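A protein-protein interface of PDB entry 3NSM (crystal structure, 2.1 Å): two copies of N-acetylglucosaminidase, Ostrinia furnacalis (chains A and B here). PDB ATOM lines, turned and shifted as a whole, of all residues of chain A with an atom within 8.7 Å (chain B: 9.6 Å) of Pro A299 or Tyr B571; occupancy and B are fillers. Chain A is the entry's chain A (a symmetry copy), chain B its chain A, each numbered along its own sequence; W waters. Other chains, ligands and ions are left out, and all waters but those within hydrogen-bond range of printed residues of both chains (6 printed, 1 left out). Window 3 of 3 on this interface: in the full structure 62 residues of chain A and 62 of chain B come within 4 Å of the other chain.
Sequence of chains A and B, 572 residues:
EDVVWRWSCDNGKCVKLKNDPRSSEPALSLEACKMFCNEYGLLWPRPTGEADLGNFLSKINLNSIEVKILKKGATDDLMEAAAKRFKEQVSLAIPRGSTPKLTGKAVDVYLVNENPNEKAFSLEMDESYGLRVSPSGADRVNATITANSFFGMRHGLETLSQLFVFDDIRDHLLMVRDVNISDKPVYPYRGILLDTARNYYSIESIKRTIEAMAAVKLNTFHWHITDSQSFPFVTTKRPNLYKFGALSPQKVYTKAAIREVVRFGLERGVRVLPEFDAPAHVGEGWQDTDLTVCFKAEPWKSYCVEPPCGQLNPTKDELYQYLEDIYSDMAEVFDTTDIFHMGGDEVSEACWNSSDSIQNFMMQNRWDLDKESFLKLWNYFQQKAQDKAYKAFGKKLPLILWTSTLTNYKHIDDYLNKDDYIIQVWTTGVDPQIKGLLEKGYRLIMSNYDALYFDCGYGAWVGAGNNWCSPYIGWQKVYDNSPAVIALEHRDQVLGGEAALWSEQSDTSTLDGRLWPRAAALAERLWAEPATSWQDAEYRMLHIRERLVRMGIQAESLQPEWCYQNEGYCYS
The side-chain hydroxyl (OH) of Tyr B571 sits at hydrogen-bond distance from the side-chain carboxylate (OE2) of Glu A298, 2.5 Å away. The indole nitrogen of Trp A300 lies within hydrogen-bond range of the backbone carbonyl oxygen of Tyr B571, 3.1 Å away. The side-chain amino group (NZ) of Lys A301 sits at hydrogen-bond distance from the side-chain hydroxyl (OG) of Ser B572.
The indole nitrogen of Trp B534 sits close to the side-chain amide nitrogen of Gln B535 (3.3 Å). The side-chain carboxylate (OE1) of Glu B538 lies close to the side-chain amide oxygen (OE1) of Gln B559, 2.9 Å away. O of Trp B562 lies close to OD1 of Asn B566, 2.8 Å away. The side-chain sulfur (SG) of Cys B570 forms a disulfide with the side-chain sulfur (SG) of Cys B563 (2.1 Å). N of Trp A300 sits at hydrogen-bond distance from OE1 of Glu A298 (3.0 Å). SG of Cys A304 is disulfide-bonded to SG of Cys A309.
Trp B562 touches Lys A296 (CZ2 to CG, 3.9 Å). Lys A296 touches Tyr B569. Tyr B571 touches Pro A299. O of Tyr B569 touches CB of Pro A307, 3.3 Å away. Trp A461 touches Pro B560. CZ3 of Trp A461 touches SG of Cys B563, at 3.8 Å. CB of Val A462 touches O of Tyr B571, at 3.8 Å. Ser B572 touches Val A462 (CB to C, 3.7 Å). Gly A463 touches Ser B572 (N to CB, 3.7 Å). Ala A464 touches Trp B534.
Pro A299 touches just one residue of chain B: Tyr B571 (3.8 Å). Glu A298 touches just one residue of chain B: Tyr B571 (2.5 Å). No residue of chain B comes within 4 Å of Ser A302. Of the printed residues of chain B, Trp A461 touches Gln B559 (3.5 Å), Pro B560 (3.5 Å) and Cys B563 (3.8 Å). Printed residues of chain A within 4 Å of Gln B559: Trp A461 (3.5 Å). Printed residues of chain B within 4 Å of Val A462: Tyr B571 (3.8 Å) and Ser B572 (3.7 Å). Asn B566 touches none of the printed residues of chain A. The nearest residue of chain A that does not touch Tyr B571 is Gly A463 (4.6 Å).
Of the 16 printed residues of chain B, 8 touch a printed residue of chain A. Among the printed residues, no Asp or Glu carboxylate lies within 4 Å of a Lys or Arg side-chain nitrogen of the other chain.
No position is printed for both chains. Of the 16 pairs that touch across the chains among the printed residues, none has its exchanged pair printed and touching as well.
Water W6 bridges the backbone carbonyl oxygen of Pro A307 (2.7 Å) and the side-chain sulfur of Cys B563 (3.6 Å). Water W3 lies within hydrogen-bond range of OE1 of Glu A298 (2.7 Å) and O of Tyr B569 (3.0 Å). Water W2 bridges the side-chain amide nitrogen of Asn B566 (2.8 Å) and the side-chain amino group of Lys A296 (3.0 Å). Water W4 bridges the backbone NH (N) of Gly A463 (3.0 Å) and the backbone NH (N) of Ser B572 (3.1 Å).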
ATOM      1  N   CYS A 294     -15.729 -24.184  23.039  1.00  0.00           N
ATOM      2  CA  CYS A 294     -16.243 -24.632  21.734  1.00  0.00           C
ATOM      3  C   CYS A 294     -15.709 -23.893  20.513  1.00  0.00           C
ATOM      4  O   CYS A 294     -16.221 -24.102  19.411  1.00  0.00           O
ATOM      5  CB  CYS A 294     -17.773 -24.566  21.662  1.00  0.00           C
ATOM      6  SG  CYS A 294     -18.666 -25.189  23.055  1.00  0.00           S
ATOM      7  N   LYS A 296     -14.447 -23.119  17.248  1.00  0.00           N
ATOM      8  CA  LYS A 296     -14.230 -23.989  16.089  1.00  0.00           C
ATOM      9  C   LYS A 296     -14.639 -25.444  16.334  1.00  0.00           C
ATOM     10  O   LYS A 296     -14.157 -26.354  15.655  1.00  0.00           O
ATOM     11  CB  LYS A 296     -12.781 -23.899  15.600  1.00  0.00           C
ATOM     12  CG  LYS A 296     -12.480 -22.634  14.840  1.00  0.00           C
ATOM     13  CD  LYS A 296     -11.066 -22.164  15.086  1.00  0.00           C
ATOM     14  CE  LYS A 296     -10.059 -22.872  14.224  1.00  0.00           C
ATOM     15  NZ  LYS A 296      -8.713 -22.289  14.469  1.00  0.00           N
ATOM     16  N   ALA A 297     -15.543 -25.652  17.290  1.00  0.00           N
ATOM     17  CA  ALA A 297     -16.044 -26.988  17.617  1.00  0.00           C
ATOM     18  C   ALA A 297     -16.615 -27.686  16.390  1.00  0.00           C
ATOM     19  O   ALA A 297     -17.346 -27.079  15.608  1.00  0.00           O
ATOM     20  CB  ALA A 297     -17.094 -26.907  18.712  1.00  0.00           C
ATOM     21  N   GLU A 298     -16.268 -28.959  16.230  1.00  0.00           N
ATOM     22  CA  GLU A 298     -16.733 -29.758  15.103  1.00  0.00           C
ATOM     23  C   GLU A 298     -17.364 -31.079  15.557  1.00  0.00           C
ATOM     24  O   GLU A 298     -16.853 -31.711  16.479  1.00  0.00           O
ATOM     25  CB  GLU A 298     -15.578 -30.021  14.140  1.00  0.00           C
ATOM     26  CG  GLU A 298     -15.376 -28.912  13.125  1.00  0.00           C
ATOM     27  CD  GLU A 298     -16.466 -28.897  12.075  1.00  0.00           C
ATOM     28  OE1 GLU A 298     -17.289 -27.962  12.075  1.00  0.00           O
ATOM     29  OE2 GLU A 298     -16.510 -29.841  11.258  1.00  0.00           O
ATOM     30  N   PRO A 299     -18.477 -31.499  14.920  1.00  0.00           N
ATOM     31  CA  PRO A 299     -19.193 -30.834  13.829  1.00  0.00           C
ATOM     32  C   PRO A 299     -19.968 -29.614  14.324  1.00  0.00           C
ATOM     33  O   PRO A 299     -20.723 -29.719  15.295  1.00  0.00           O
ATOM     34  CB  PRO A 299     -20.163 -31.915  13.341  1.00  0.00           C
ATOM     35  CG  PRO A 299     -20.434 -32.735  14.551  1.00  0.00           C
ATOM     36  CD  PRO A 299     -19.128 -32.767  15.301  1.00  0.00           C
ATOM     37  N   TRP A 300     -19.782 -28.474  13.654  1.00  0.00           N
ATOM     38  CA  TRP A 300     -20.372 -27.201  14.097  1.00  0.00           C
ATOM     39  C   TRP A 300     -21.889 -27.240  14.259  1.00  0.00           C
ATOM     40  O   TRP A 300     -22.445 -26.525  15.092  1.00  0.00           O
ATOM     41  CB  TRP A 300     -19.959 -26.042  13.179  1.00  0.00           C
ATOM     42  CG  TRP A 300     -20.543 -26.077  11.787  1.00  0.00           C
ATOM     43  CD1 TRP A 300     -19.943 -26.560  10.662  1.00  0.00           C
ATOM     44  CD2 TRP A 300     -21.832 -25.590  11.376  1.00  0.00           C
ATOM     45  NE1 TRP A 300     -20.773 -26.412   9.580  1.00  0.00           N
ATOM     46  CE2 TRP A 300     -21.939 -25.820   9.989  1.00  0.00           C
ATOM     47  CE3 TRP A 300     -22.904 -24.980  12.046  1.00  0.00           C
ATOM     48  CZ2 TRP A 300     -23.078 -25.467   9.255  1.00  0.00           C
ATOM     49  CZ3 TRP A 300     -24.039 -24.632  11.316  1.00  0.00           C
ATOM     50  CH2 TRP A 300     -24.114 -24.875   9.934  1.00  0.00           C
ATOM     51  N   LYS A 301     -22.541 -28.086  13.466  1.00  0.00           N
ATOM     52  CA  LYS A 301     -23.996 -28.212  13.452  1.00  0.00           C
ATOM     53  C   LYS A 301     -24.578 -28.663  14.798  1.00  0.00           C
ATOM     54  O   LYS A 301     -25.758 -28.440  15.082  1.00  0.00           O
ATOM     55  CB  LYS A 301     -24.407 -29.191  12.355  1.00  0.00           C
ATOM     56  CG  LYS A 301     -25.525 -28.691  11.468  1.00  0.00           C
ATOM     57  CD  LYS A 301     -25.389 -29.265  10.060  1.00  0.00           C
ATOM     58  CE  LYS A 301     -26.018 -28.349   9.015  1.00  0.00           C
ATOM     59  NZ  LYS A 301     -25.564 -28.720   7.641  1.00  0.00           N
ATOM     60  N   SER A 302     -23.738 -29.283  15.623  1.00  0.00           N
ATOM     61  CA  SER A 302     -24.169 -29.811  16.915  1.00  0.00           C
ATOM     62  C   SER A 302     -24.040 -28.796  18.051  1.00  0.00           C
ATOM     63  O   SER A 302     -24.622 -28.983  19.125  1.00  0.00           O
ATOM     64  CB  SER A 302     -23.373 -31.073  17.251  1.00  0.00           C
ATOM     65  OG  SER A 302     -23.480 -32.028  16.211  1.00  0.00           O
ATOM     66  N   TYR A 303     -23.287 -27.723  17.811  1.00  0.00           N
ATOM     67  CA  TYR A 303     -22.900 -26.808  18.882  1.00  0.00           C
ATOM     68  C   TYR A 303     -23.319 -25.356  18.679  1.00  0.00           C
ATOM     69  O   TYR A 303     -23.388 -24.599  19.648  1.00  0.00           O
ATOM     70  CB  TYR A 303     -21.389 -26.874  19.126  1.00  0.00           C
ATOM     71  CG  TYR A 303     -20.892 -28.243  19.510  1.00  0.00           C
ATOM     72  CD1 TYR A 303     -21.003 -28.707  20.824  1.00  0.00           C
ATOM     73  CD2 TYR A 303     -20.314 -29.081  18.558  1.00  0.00           C
ATOM     74  CE1 TYR A 303     -20.547 -29.980  21.179  1.00  0.00           C
ATOM     75  CE2 TYR A 303     -19.857 -30.350  18.898  1.00  0.00           C
ATOM     76  CZ  TYR A 303     -19.974 -30.794  20.207  1.00  0.00           C
ATOM     77  OH  TYR A 303     -19.511 -32.053  20.532  1.00  0.00           O
ATOM     78  N   CYS A 304     -23.578 -24.955  17.437  1.00  0.00           N
ATOM     79  CA  CYS A 304     -23.940 -23.559  17.173  1.00  0.00           C
ATOM     80  C   CYS A 304     -24.783 -23.354  15.913  1.00  0.00           C
ATOM     81  O   CYS A 304     -24.906 -24.253  15.073  1.00  0.00           O
ATOM     82  CB  CYS A 304     -22.686 -22.670  17.145  1.00  0.00           C
ATOM     83  SG  CYS A 304     -21.552 -23.045  15.803  1.00  0.00           S
ATOM     84  N   VAL A 305     -25.353 -22.153  15.805  1.00  0.00           N
ATOM     85  CA  VAL A 305     -26.213 -21.755  14.690  1.00  0.00           C
ATOM     86  C   VAL A 305     -25.447 -21.685  13.365  1.00  0.00           C
ATOM     87  O   VAL A 305     -25.971 -22.086  12.327  1.00  0.00           O
ATOM     88  CB  VAL A 305     -26.906 -20.393  14.979  1.00  0.00           C
ATOM     89  CG1 VAL A 305     -27.806 -19.977  13.831  1.00  0.00           C
ATOM     90  CG2 VAL A 305     -27.719 -20.473  16.265  1.00  0.00           C
ATOM     91  N   GLU A 306     -24.215 -21.182  13.408  1.00  0.00           N
ATOM     92  CA  GLU A 306     -23.379 -21.039  12.211  1.00  0.00           C
ATOM     93  C   GLU A 306     -21.893 -21.090  12.588  1.00  0.00           C
ATOM     94  O   GLU A 306     -21.519 -20.655  13.674  1.00  0.00           O
ATOM     95  CB  GLU A 306     -23.716 -19.738  11.445  1.00  0.00           C
ATOM     96  CG  GLU A 306     -23.316 -18.438  12.155  1.00  0.00           C
ATOM     97  CD  GLU A 306     -23.640 -17.173  11.358  1.00  0.00           C
ATOM     98  OE1 GLU A 306     -22.728 -16.335  11.163  1.00  0.00           O
ATOM     99  OE2 GLU A 306     -24.800 -17.018  10.930  1.00  0.00           O
ATOM    100  N   PRO A 307     -21.042 -21.631  11.696  1.00  0.00           N
ATOM    101  CA  PRO A 307     -19.618 -21.698  12.018  1.00  0.00           C
ATOM    102  C   PRO A 307     -18.980 -20.310  11.964  1.00  0.00           C
ATOM    103  O   PRO A 307     -19.394 -19.485  11.152  1.00  0.00           O
ATOM    104  CB  PRO A 307     -19.055 -22.587  10.915  1.00  0.00           C
ATOM    105  CG  PRO A 307     -19.975 -22.387   9.765  1.00  0.00           C
ATOM    106  CD  PRO A 307     -21.333 -22.183  10.361  1.00  0.00           C
ATOM    107  N   CYS A 309     -18.256 -22.077  15.812  1.00  0.00           N
ATOM    108  CA  CYS A 309     -18.836 -22.106  17.153  1.00  0.00           C
ATOM    109  C   CYS A 309     -17.897 -21.406  18.129  1.00  0.00           C
ATOM    110  O   CYS A 309     -16.728 -21.171  17.811  1.00  0.00           O
ATOM    111  CB  CYS A 309     -19.127 -23.543  17.598  1.00  0.00           C
ATOM    112  SG  CYS A 309     -20.285 -24.460  16.537  1.00  0.00           S
ATOM    113  N   ALA A 350     -25.626 -27.143  24.446  1.00  0.00           N
ATOM    114  CA  ALA A 350     -24.693 -28.224  24.146  1.00  0.00           C
ATOM    115  C   ALA A 350     -23.257 -27.756  24.305  1.00  0.00           C
ATOM    116  O   ALA A 350     -22.401 -28.496  24.796  1.00  0.00           O
ATOM    117  CB  ALA A 350     -24.921 -28.744  22.735  1.00  0.00           C
ATOM    118  N   TRP A 461     -24.465 -19.614   1.846  1.00  0.00           N
ATOM    119  CA  TRP A 461     -23.032 -19.434   2.119  1.00  0.00           C
ATOM    120  C   TRP A 461     -22.406 -20.681   2.758  1.00  0.00           C
ATOM    121  O   TRP A 461     -21.182 -20.820   2.806  1.00  0.00           O
ATOM    122  CB  TRP A 461     -22.742 -18.162   2.923  1.00  0.00           C
ATOM    123  CG  TRP A 461     -23.231 -18.127   4.345  1.00  0.00           C
ATOM    124  CD1 TRP A 461     -24.450 -17.686   4.785  1.00  0.00           C
ATOM    125  CD2 TRP A 461     -22.492 -18.495   5.519  1.00  0.00           C
ATOM    126  NE1 TRP A 461     -24.523 -17.775   6.153  1.00  0.00           N
ATOM    127  CE2 TRP A 461     -23.337 -18.266   6.633  1.00  0.00           C
ATOM    128  CE3 TRP A 461     -21.201 -19.005   5.738  1.00  0.00           C
ATOM    129  CZ2 TRP A 461     -22.933 -18.530   7.951  1.00  0.00           C
ATOM    130  CZ3 TRP A 461     -20.795 -19.266   7.055  1.00  0.00           C
ATOM    131  CH2 TRP A 461     -21.659 -19.026   8.141  1.00  0.00           C
ATOM    132  N   VAL A 462     -23.262 -21.571   3.255  1.00  0.00           N
ATOM    133  CA  VAL A 462     -22.864 -22.944   3.552  1.00  0.00           C
ATOM    134  C   VAL A 462     -23.721 -23.876   2.702  1.00  0.00           C
ATOM    135  O   VAL A 462     -24.951 -23.812   2.730  1.00  0.00           O
ATOM    136  CB  VAL A 462     -22.944 -23.309   5.068  1.00  0.00           C
ATOM    137  CG1 VAL A 462     -21.906 -22.535   5.856  1.00  0.00           C
ATOM    138  CG2 VAL A 462     -24.342 -23.078   5.644  1.00  0.00           C
ATOM    139  N   GLY A 463     -23.066 -24.723   1.920  1.00  0.00           N
ATOM    140  CA  GLY A 463     -23.776 -25.612   1.004  1.00  0.00           C
ATOM    141  C   GLY A 463     -24.348 -24.823  -0.159  1.00  0.00           C
ATOM    142  O   GLY A 463     -23.819 -23.763  -0.520  1.00  0.00           O
ATOM    143  N   ALA A 464     -25.428 -25.335  -0.743  1.00  0.00           N
ATOM    144  CA  ALA A 464     -26.016 -24.736  -1.936  1.00  0.00           C
ATOM    145  C   ALA A 464     -27.471 -24.367  -1.698  1.00  0.00           C
ATOM    146  O   ALA A 464     -28.014 -24.651  -0.633  1.00  0.00           O
ATOM    147  CB  ALA A 464     -25.878 -25.681  -3.131  1.00  0.00           C
ATOM    148  N   LYS B  13      -6.507 -28.037   2.696  1.00  0.00           N
ATOM    149  CA  LYS B  13      -7.039 -26.863   3.383  1.00  0.00           C
ATOM    150  C   LYS B  13      -5.917 -26.095   4.068  1.00  0.00           C
ATOM    151  O   LYS B  13      -5.075 -26.688   4.744  1.00  0.00           O
ATOM    152  CB  LYS B  13      -8.080 -27.287   4.424  1.00  0.00           C
ATOM    153  CG  LYS B  13      -9.233 -28.127   3.864  1.00  0.00           C
ATOM    154  CD  LYS B  13     -10.098 -28.736   4.967  1.00  0.00           C
ATOM    155  CE  LYS B  13      -9.381 -29.891   5.671  1.00  0.00           C
ATOM    156  NZ  LYS B  13     -10.333 -30.790   6.391  1.00  0.00           N
ATOM    157  N   TRP B 534     -19.265 -27.585  -7.912  1.00  0.00           N
ATOM    158  CA  TRP B 534     -18.949 -26.270  -7.368  1.00  0.00           C
ATOM    159  C   TRP B 534     -18.062 -26.312  -6.123  1.00  0.00           C
ATOM    160  O   TRP B 534     -17.177 -25.467  -5.966  1.00  0.00           O
ATOM    161  CB  TRP B 534     -20.224 -25.452  -7.125  1.00  0.00           C
ATOM    162  CG  TRP B 534     -21.113 -25.917  -5.991  1.00  0.00           C
ATOM    163  CD1 TRP B 534     -22.241 -26.688  -6.093  1.00  0.00           C
ATOM    164  CD2 TRP B 534     -20.965 -25.610  -4.595  1.00  0.00           C
ATOM    165  NE1 TRP B 534     -22.796 -26.886  -4.852  1.00  0.00           N
ATOM    166  CE2 TRP B 534     -22.034 -26.238  -3.915  1.00  0.00           C
ATOM    167  CE3 TRP B 534     -20.035 -24.865  -3.855  1.00  0.00           C
ATOM    168  CZ2 TRP B 534     -22.197 -26.149  -2.529  1.00  0.00           C
ATOM    169  CZ3 TRP B 534     -20.196 -24.777  -2.475  1.00  0.00           C
ATOM    170  CH2 TRP B 534     -21.270 -25.418  -1.828  1.00  0.00           C
ATOM    171  N   GLN B 535     -18.279 -27.305  -5.258  1.00  0.00           N
ATOM    172  CA  GLN B 535     -17.523 -27.402  -4.007  1.00  0.00           C
ATOM    173  C   GLN B 535     -16.027 -27.590  -4.225  1.00  0.00           C
ATOM    174  O   GLN B 535     -15.231 -27.216  -3.371  1.00  0.00           O
ATOM    175  CB  GLN B 535     -18.092 -28.455  -3.043  1.00  0.00           C
ATOM    176  CG  GLN B 535     -18.737 -29.653  -3.688  1.00  0.00           C
ATOM    177  CD  GLN B 535     -20.237 -29.484  -3.859  1.00  0.00           C
ATOM    178  OE1 GLN B 535     -20.983 -29.381  -2.881  1.00  0.00           O
ATOM    179  NE2 GLN B 535     -20.686 -29.470  -5.106  1.00  0.00           N
ATOM    180  N   GLU B 538     -14.942 -23.968  -4.947  1.00  0.00           N
ATOM    181  CA  GLU B 538     -15.284 -23.029  -3.875  1.00  0.00           C
ATOM    182  C   GLU B 538     -14.143 -22.121  -3.420  1.00  0.00           C
ATOM    183  O   GLU B 538     -14.280 -20.904  -3.460  1.00  0.00           O
ATOM    184  CB  GLU B 538     -15.879 -23.763  -2.667  1.00  0.00           C
ATOM    185  CG  GLU B 538     -16.438 -22.819  -1.593  1.00  0.00           C
ATOM    186  CD  GLU B 538     -16.897 -23.530  -0.325  1.00  0.00           C
ATOM    187  OE1 GLU B 538     -17.191 -22.835   0.675  1.00  0.00           O
ATOM    188  OE2 GLU B 538     -16.969 -24.775  -0.314  1.00  0.00           O
ATOM    189  N   TYR B 539     -13.025 -22.708  -2.995  1.00  0.00           N
ATOM    190  CA  TYR B 539     -11.907 -21.919  -2.464  1.00  0.00           C
ATOM    191  C   TYR B 539     -11.381 -20.913  -3.477  1.00  0.00           C
ATOM    192  O   TYR B 539     -11.149 -19.758  -3.132  1.00  0.00           O
ATOM    193  CB  TYR B 539     -10.760 -22.812  -1.951  1.00  0.00           C
ATOM    194  CG  TYR B 539     -11.155 -23.813  -0.884  1.00  0.00           C
ATOM    195  CD1 TYR B 539     -10.335 -24.907  -0.589  1.00  0.00           C
ATOM    196  CD2 TYR B 539     -12.354 -23.677  -0.173  1.00  0.00           C
ATOM    197  CE1 TYR B 539     -10.693 -25.832   0.383  1.00  0.00           C
ATOM    198  CE2 TYR B 539     -12.725 -24.601   0.794  1.00  0.00           C
ATOM    199  CZ  TYR B 539     -11.892 -25.675   1.066  1.00  0.00           C
ATOM    200  OH  TYR B 539     -12.257 -26.578   2.033  1.00  0.00           O
ATOM    201  N   GLN B 559     -19.373 -15.217   1.199  1.00  0.00           N
ATOM    202  CA  GLN B 559     -19.169 -15.857   2.496  1.00  0.00           C
ATOM    203  C   GLN B 559     -18.407 -14.915   3.407  1.00  0.00           C
ATOM    204  O   GLN B 559     -17.783 -13.971   2.928  1.00  0.00           O
ATOM    205  CB  GLN B 559     -18.366 -17.159   2.336  1.00  0.00           C
ATOM    206  CG  GLN B 559     -19.089 -18.259   1.566  1.00  0.00           C
ATOM    207  CD  GLN B 559     -18.284 -19.551   1.426  1.00  0.00           C
ATOM    208  OE1 GLN B 559     -18.426 -20.264   0.437  1.00  0.00           O
ATOM    209  NE2 GLN B 559     -17.454 -19.856   2.412  1.00  0.00           N
ATOM    210  N   PRO B 560     -18.452 -15.155   4.731  1.00  0.00           N
ATOM    211  CA  PRO B 560     -17.592 -14.377   5.616  1.00  0.00           C
ATOM    212  C   PRO B 560     -16.129 -14.553   5.214  1.00  0.00           C
ATOM    213  O   PRO B 560     -15.730 -15.648   4.796  1.00  0.00           O
ATOM    214  CB  PRO B 560     -17.831 -15.013   6.979  1.00  0.00           C
ATOM    215  CG  PRO B 560     -19.190 -15.608   6.885  1.00  0.00           C
ATOM    216  CD  PRO B 560     -19.306 -16.096   5.478  1.00  0.00           C
ATOM    217  N   TRP B 562     -13.826 -14.771   7.152  1.00  0.00           N
ATOM    218  CA  TRP B 562     -13.384 -15.810   8.066  1.00  0.00           C
ATOM    219  C   TRP B 562     -13.331 -17.178   7.383  1.00  0.00           C
ATOM    220  O   TRP B 562     -12.419 -17.961   7.655  1.00  0.00           O
ATOM    221  CB  TRP B 562     -14.263 -15.891   9.317  1.00  0.00           C
ATOM    222  CG  TRP B 562     -13.684 -16.807  10.358  1.00  0.00           C
ATOM    223  CD1 TRP B 562     -12.816 -16.470  11.356  1.00  0.00           C
ATOM    224  CD2 TRP B 562     -13.909 -18.219  10.482  1.00  0.00           C
ATOM    225  NE1 TRP B 562     -12.487 -17.582  12.095  1.00  0.00           N
ATOM    226  CE2 TRP B 562     -13.141 -18.669  11.579  1.00  0.00           C
ATOM    227  CE3 TRP B 562     -14.684 -19.149   9.770  1.00  0.00           C
ATOM    228  CZ2 TRP B 562     -13.127 -20.011  11.989  1.00  0.00           C
ATOM    229  CZ3 TRP B 562     -14.671 -20.481  10.176  1.00  0.00           C
ATOM    230  CH2 TRP B 562     -13.900 -20.896  11.279  1.00  0.00           C
ATOM    231  N   CYS B 563     -14.292 -17.458   6.501  1.00  0.00           N
ATOM    232  CA  CYS B 563     -14.339 -18.752   5.807  1.00  0.00           C
ATOM    233  C   CYS B 563     -13.176 -18.906   4.821  1.00  0.00           C
ATOM    234  O   CYS B 563     -12.642 -20.002   4.648  1.00  0.00           O
ATOM    235  CB  CYS B 563     -15.664 -18.939   5.074  1.00  0.00           C
ATOM    236  SG  CYS B 563     -17.127 -19.005   6.146  1.00  0.00           S
ATOM    237  N   ASN B 566     -10.139 -19.676   6.746  1.00  0.00           N
ATOM    238  CA  ASN B 566     -10.269 -20.895   7.535  1.00  0.00           C
ATOM    239  C   ASN B 566     -10.945 -22.008   6.755  1.00  0.00           C
ATOM    240  O   ASN B 566     -11.993 -22.518   7.155  1.00  0.00           O
ATOM    241  CB  ASN B 566     -11.028 -20.610   8.836  1.00  0.00           C
ATOM    242  CG  ASN B 566     -10.282 -19.650   9.742  1.00  0.00           C
ATOM    243  OD1 ASN B 566     -10.535 -18.443   9.731  1.00  0.00           O
ATOM    244  ND2 ASN B 566      -9.349 -20.174  10.521  1.00  0.00           N
ATOM    245  N   GLU B 567     -10.333 -22.370   5.633  1.00  0.00           N
ATOM    246  CA  GLU B 567     -10.861 -23.406   4.740  1.00  0.00           C
ATOM    247  C   GLU B 567     -11.281 -24.677   5.461  1.00  0.00           C
ATOM    248  O   GLU B 567     -10.530 -25.220   6.267  1.00  0.00           O
ATOM    249  CB  GLU B 567      -9.844 -23.731   3.644  1.00  0.00           C
ATOM    250  CG  GLU B 567      -9.789 -22.665   2.564  1.00  0.00           C
ATOM    251  CD  GLU B 567      -8.609 -22.811   1.621  1.00  0.00           C
ATOM    252  OE1 GLU B 567      -8.588 -22.080   0.607  1.00  0.00           O
ATOM    253  OE2 GLU B 567      -7.707 -23.642   1.883  1.00  0.00           O
ATOM    254  N   GLY B 568     -12.496 -25.135   5.175  1.00  0.00           N
ATOM    255  CA  GLY B 568     -12.986 -26.392   5.720  1.00  0.00           C
ATOM    256  C   GLY B 568     -13.946 -26.262   6.883  1.00  0.00           C
ATOM    257  O   GLY B 568     -14.706 -27.186   7.166  1.00  0.00           O
ATOM    258  N   TYR B 569     -13.926 -25.124   7.565  1.00  0.00           N
ATOM    259  CA  TYR B 569     -14.812 -24.942   8.708  1.00  0.00           C
ATOM    260  C   TYR B 569     -16.218 -24.480   8.328  1.00  0.00           C
ATOM    261  O   TYR B 569     -17.155 -24.665   9.104  1.00  0.00           O
ATOM    262  CB  TYR B 569     -14.195 -23.996   9.731  1.00  0.00           C
ATOM    263  CG  TYR B 569     -13.068 -24.609  10.535  1.00  0.00           C
ATOM    264  CD1 TYR B 569     -11.737 -24.419  10.160  1.00  0.00           C
ATOM    265  CD2 TYR B 569     -13.331 -25.361  11.683  1.00  0.00           C
ATOM    266  CE1 TYR B 569     -10.699 -24.966  10.895  1.00  0.00           C
ATOM    267  CE2 TYR B 569     -12.302 -25.910  12.428  1.00  0.00           C
ATOM    268  CZ  TYR B 569     -10.986 -25.711  12.024  1.00  0.00           C
ATOM    269  OH  TYR B 569      -9.953 -26.255  12.754  1.00  0.00           O
ATOM    270  N   CYS B 570     -16.360 -23.875   7.150  1.00  0.00           N
ATOM    271  CA  CYS B 570     -17.669 -23.452   6.648  1.00  0.00           C
ATOM    272  C   CYS B 570     -18.147 -24.440   5.584  1.00  0.00           C
ATOM    273  O   CYS B 570     -17.654 -24.428   4.454  1.00  0.00           O
ATOM    274  CB  CYS B 570     -17.603 -22.034   6.070  1.00  0.00           C
ATOM    275  SG  CYS B 570     -16.945 -20.771   7.198  1.00  0.00           S
ATOM    276  N   TYR B 571     -19.091 -25.303   5.950  1.00  0.00           N
ATOM    277  CA  TYR B 571     -19.579 -26.355   5.050  1.00  0.00           C
ATOM    278  C   TYR B 571     -21.004 -26.791   5.410  1.00  0.00           C
ATOM    279  O   TYR B 571     -21.472 -26.543   6.525  1.00  0.00           O
ATOM    280  CB  TYR B 571     -18.647 -27.573   5.099  1.00  0.00           C
ATOM    281  CG  TYR B 571     -18.671 -28.270   6.440  1.00  0.00           C
ATOM    282  CD1 TYR B 571     -17.766 -27.925   7.441  1.00  0.00           C
ATOM    283  CD2 TYR B 571     -19.619 -29.257   6.718  1.00  0.00           C
ATOM    284  CE1 TYR B 571     -17.793 -28.546   8.680  1.00  0.00           C
ATOM    285  CE2 TYR B 571     -19.656 -29.887   7.960  1.00  0.00           C
ATOM    286  CZ  TYR B 571     -18.739 -29.529   8.934  1.00  0.00           C
ATOM    287  OH  TYR B 571     -18.772 -30.150  10.161  1.00  0.00           O
ATOM    288  N   SER B 572     -21.680 -27.448   4.465  1.00  0.00           N
ATOM    289  CA  SER B 572     -23.000 -28.045   4.703  1.00  0.00           C
ATOM    290  C   SER B 572     -23.322 -29.103   3.650  1.00  0.00           C
ATOM    291  O   SER B 572     -23.428 -30.296   3.963  1.00  0.00           O
ATOM    292  CB  SER B 572     -24.094 -26.979   4.723  1.00  0.00           C
ATOM    293  OG  SER B 572     -25.347 -27.559   5.020  1.00  0.00           O
HETATM  294  O   HOH W   1     -21.341 -29.719  10.955  1.00  0.00           O
HETATM  295  O   HOH W   2      -9.525 -19.708  13.267  1.00  0.00           O
HETATM  296  O   HOH W   3     -16.858 -25.310  11.999  1.00  0.00           O
HETATM  297  O   HOH W   4     -20.531 -26.305   1.865  1.00  0.00           O
HETATM  298  O   HOH W   5     -23.493 -30.849   7.302  1.00  0.00           O
HETATM  299  O   HOH W   6     -18.155 -17.890   9.387  1.00  0.00           O
